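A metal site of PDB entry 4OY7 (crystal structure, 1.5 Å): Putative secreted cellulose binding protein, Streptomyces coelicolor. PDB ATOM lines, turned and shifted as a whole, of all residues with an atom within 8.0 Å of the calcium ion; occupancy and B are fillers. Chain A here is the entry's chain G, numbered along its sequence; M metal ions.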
ATOM      1  N   ASP A  17      -1.241  26.751 -21.344  1.00  0.00           N
ATOM      2  CA  ASP A  17      -0.121  26.892 -20.367  1.00  0.00           C
ATOM      3  C   ASP A  17       0.622  25.556 -20.222  1.00  0.00           C
ATOM      4  O   ASP A  17       1.821  25.525 -19.999  1.00  0.00           O
ATOM      5  CB  ASP A  17      -0.713  27.343 -19.025  1.00  0.00           C
ATOM      6  CG  ASP A  17       0.317  27.826 -18.011  1.00  0.00           C
ATOM      7  OD1 ASP A  17       0.581  27.099 -17.057  1.00  0.00           O
ATOM      8  OD2 ASP A  17       0.803  28.970 -18.142  1.00  0.00           O
ATOM      9  N   ALA A  18      -0.127  24.455 -20.338  1.00  0.00           N
ATOM     10  CA  ALA A  18       0.414  23.114 -20.126  1.00  0.00           C
ATOM     11  C   ALA A  18       1.119  22.533 -21.356  1.00  0.00           C
ATOM     12  O   ALA A  18       1.850  21.557 -21.217  1.00  0.00           O
ATOM     13  CB  ALA A  18      -0.697  22.179 -19.692  1.00  0.00           C
ATOM     14  N   LEU A  25       1.636  17.210 -20.592  1.00  0.00           N
ATOM     15  CA  LEU A  25       1.078  18.398 -19.975  1.00  0.00           C
ATOM     16  C   LEU A  25       1.910  18.813 -18.785  1.00  0.00           C
ATOM     17  O   LEU A  25       2.046  18.049 -17.829  1.00  0.00           O
ATOM     18  CB  LEU A  25      -0.335  18.090 -19.522  1.00  0.00           C
ATOM     19  CG  LEU A  25      -1.321  17.668 -20.616  1.00  0.00           C
ATOM     20  CD1 LEU A  25      -2.613  17.116 -20.006  1.00  0.00           C
ATOM     21  CD2 LEU A  25      -1.634  18.817 -21.566  1.00  0.00           C
ATOM     22  N   ASP A  26       2.485  20.014 -18.859  1.00  0.00           N
ATOM     23  CA  ASP A  26       3.185  20.584 -17.720  1.00  0.00           C
ATOM     24  C   ASP A  26       3.003  22.094 -17.629  1.00  0.00           C
ATOM     25  O   ASP A  26       3.822  22.861 -18.127  1.00  0.00           O
ATOM     26  CB  ASP A  26       4.671  20.237 -17.757  1.00  0.00           C
ATOM     27  CG  ASP A  26       5.371  20.533 -16.448  1.00  0.00           C
ATOM     28  OD1 ASP A  26       4.711  21.091 -15.515  1.00  0.00           O
ATOM     29  OD2 ASP A  26       6.587  20.261 -16.332  1.00  0.00           O
ATOM     30  N   PRO A  27       1.945  22.537 -16.922  1.00  0.00           N
ATOM     31  CA  PRO A  27       1.736  23.982 -16.779  1.00  0.00           C
ATOM     32  C   PRO A  27       2.705  24.639 -15.778  1.00  0.00           C
ATOM     33  O   PRO A  27       3.153  23.992 -14.843  1.00  0.00           O
ATOM     34  CB  PRO A  27       0.327  24.060 -16.235  1.00  0.00           C
ATOM     35  CG  PRO A  27       0.167  22.824 -15.433  1.00  0.00           C
ATOM     36  CD  PRO A  27       0.890  21.764 -16.236  1.00  0.00           C
ATOM     37  N   THR A  28       3.014  25.895 -15.999  1.00  0.00           N
ATOM     38  CA  THR A  28       3.799  26.671 -15.057  1.00  0.00           C
ATOM     39  C   THR A  28       2.900  27.397 -14.074  1.00  0.00           C
ATOM     40  O   THR A  28       3.312  27.666 -12.968  1.00  0.00           O
ATOM     41  CB  THR A  28       4.766  27.674 -15.737  1.00  0.00           C
ATOM     42  OG1 THR A  28       4.046  28.604 -16.544  1.00  0.00           O
ATOM     43  CG2 THR A  28       5.780  26.964 -16.582  1.00  0.00           C
ATOM     44  N   ASN A  29       1.670  27.691 -14.460  1.00  0.00           N
ATOM     45  CA  ASN A  29       0.759  28.410 -13.561  1.00  0.00           C
ATOM     46  C   ASN A  29       0.342  27.498 -12.396  1.00  0.00           C
ATOM     47  O   ASN A  29      -0.033  26.352 -12.598  1.00  0.00           O
ATOM     48  CB  ASN A  29      -0.451  28.930 -14.311  1.00  0.00           C
ATOM     49  CG  ASN A  29      -1.504  29.511 -13.382  1.00  0.00           C
ATOM     50  OD1 ASN A  29      -2.292  28.789 -12.778  1.00  0.00           O
ATOM     51  ND2 ASN A  29      -1.557  30.833 -13.294  1.00  0.00           N
ATOM     52  N   PRO A  30       0.451  27.994 -11.152  1.00  0.00           N
ATOM     53  CA  PRO A  30       0.173  27.113  -9.981  1.00  0.00           C
ATOM     54  C   PRO A  30      -1.289  26.637  -9.810  1.00  0.00           C
ATOM     55  O   PRO A  30      -1.509  25.524  -9.316  1.00  0.00           O
ATOM     56  CB  PRO A  30       0.668  27.940  -8.807  1.00  0.00           C
ATOM     57  CG  PRO A  30       0.637  29.337  -9.273  1.00  0.00           C
ATOM     58  CD  PRO A  30       0.951  29.318 -10.744  1.00  0.00           C
ATOM     59  N   CYS A  32      -3.237  26.036 -12.454  1.00  0.00           N
ATOM     60  CA  CYS A  32      -3.375  25.031 -13.524  1.00  0.00           C
ATOM     61  C   CYS A  32      -2.677  23.740 -13.107  1.00  0.00           C
ATOM     62  O   CYS A  32      -3.185  22.644 -13.335  1.00  0.00           O
ATOM     63  CB  CYS A  32      -2.773  25.518 -14.838  1.00  0.00           C
ATOM     64  SG  CYS A  32      -3.582  26.920 -15.610  1.00  0.00           S
ATOM     65  N   GLN A  33      -1.508  23.851 -12.493  1.00  0.00           N
ATOM     66  CA  GLN A  33      -0.851  22.656 -11.989  1.00  0.00           C
ATOM     67  C   GLN A  33      -1.671  21.948 -10.935  1.00  0.00           C
ATOM     68  O   GLN A  33      -1.797  20.703 -10.959  1.00  0.00           O
ATOM     69  CB  GLN A  33       0.511  23.020 -11.383  1.00  0.00           C
ATOM     70  CG  GLN A  33       1.383  21.828 -11.012  1.00  0.00           C
ATOM     71  CD  GLN A  33       1.819  21.046 -12.229  1.00  0.00           C
ATOM     72  OE1 GLN A  33       2.465  21.573 -13.142  1.00  0.00           O
ATOM     73  NE2 GLN A  33       1.433  19.769 -12.276  1.00  0.00           N
ATOM     74  N   ALA A  34      -2.242  22.696  -9.996  1.00  0.00           N
ATOM     75  CA  ALA A  34      -3.104  22.079  -8.997  1.00  0.00           C
ATOM     76  C   ALA A  34      -4.278  21.365  -9.650  1.00  0.00           C
ATOM     77  O   ALA A  34      -4.667  20.272  -9.226  1.00  0.00           O
ATOM     78  CB  ALA A  34      -3.571  23.119  -7.987  1.00  0.00           C
ATOM     79  N   LEU A  36      -4.423  20.101 -12.691  1.00  0.00           N
ATOM     80  CA  LEU A  36      -3.930  18.896 -13.381  1.00  0.00           C
ATOM     81  C   LEU A  36      -3.693  17.792 -12.363  1.00  0.00           C
ATOM     82  O   LEU A  36      -4.075  16.638 -12.575  1.00  0.00           O
ATOM     83  CB  LEU A  36      -2.639  19.189 -14.143  1.00  0.00           C
ATOM     84  CG  LEU A  36      -1.943  18.022 -14.846  1.00  0.00           C
ATOM     85  CD1 LEU A  36      -2.872  17.378 -15.852  1.00  0.00           C
ATOM     86  CD2 LEU A  36      -0.693  18.549 -15.528  1.00  0.00           C
ATOM     87  N   ASP A  37      -3.077  18.161 -11.245  1.00  0.00           N
ATOM     88  CA  ASP A  37      -2.781  17.216 -10.190  1.00  0.00           C
ATOM     89  C   ASP A  37      -4.043  16.604  -9.607  1.00  0.00           C
ATOM     90  O   ASP A  37      -4.066  15.400  -9.355  1.00  0.00           O
ATOM     91  CB  ASP A  37      -1.974  17.894  -9.088  1.00  0.00           C
ATOM     92  CG  ASP A  37      -0.550  18.234  -9.530  1.00  0.00           C
ATOM     93  OD1 ASP A  37       0.074  18.990  -8.802  1.00  0.00           O
ATOM     94  OD2 ASP A  37      -0.038  17.746 -10.591  1.00  0.00           O
HETATM   95 CA    CA M   1       4.482  22.465 -13.700  1.00  0.00          CA
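Of the 13 residues printed, 3 come within 4 Å of the calcium ion.
The backbone NH (N) of Asp 26 sits at hydrogen-bond distance from the backbone carbonyl oxygen (O) of Ala 18. OD2 of Asp 37 lies within hydrogen-bond range of NE2 of Gln 33 (3.0 Å).
The calcium ion is bound by OE1 of Gln 33 (2.3 Å), OD1 of Asp 26 (2.3 Å) and O of Pro 27 (2.3 Å).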
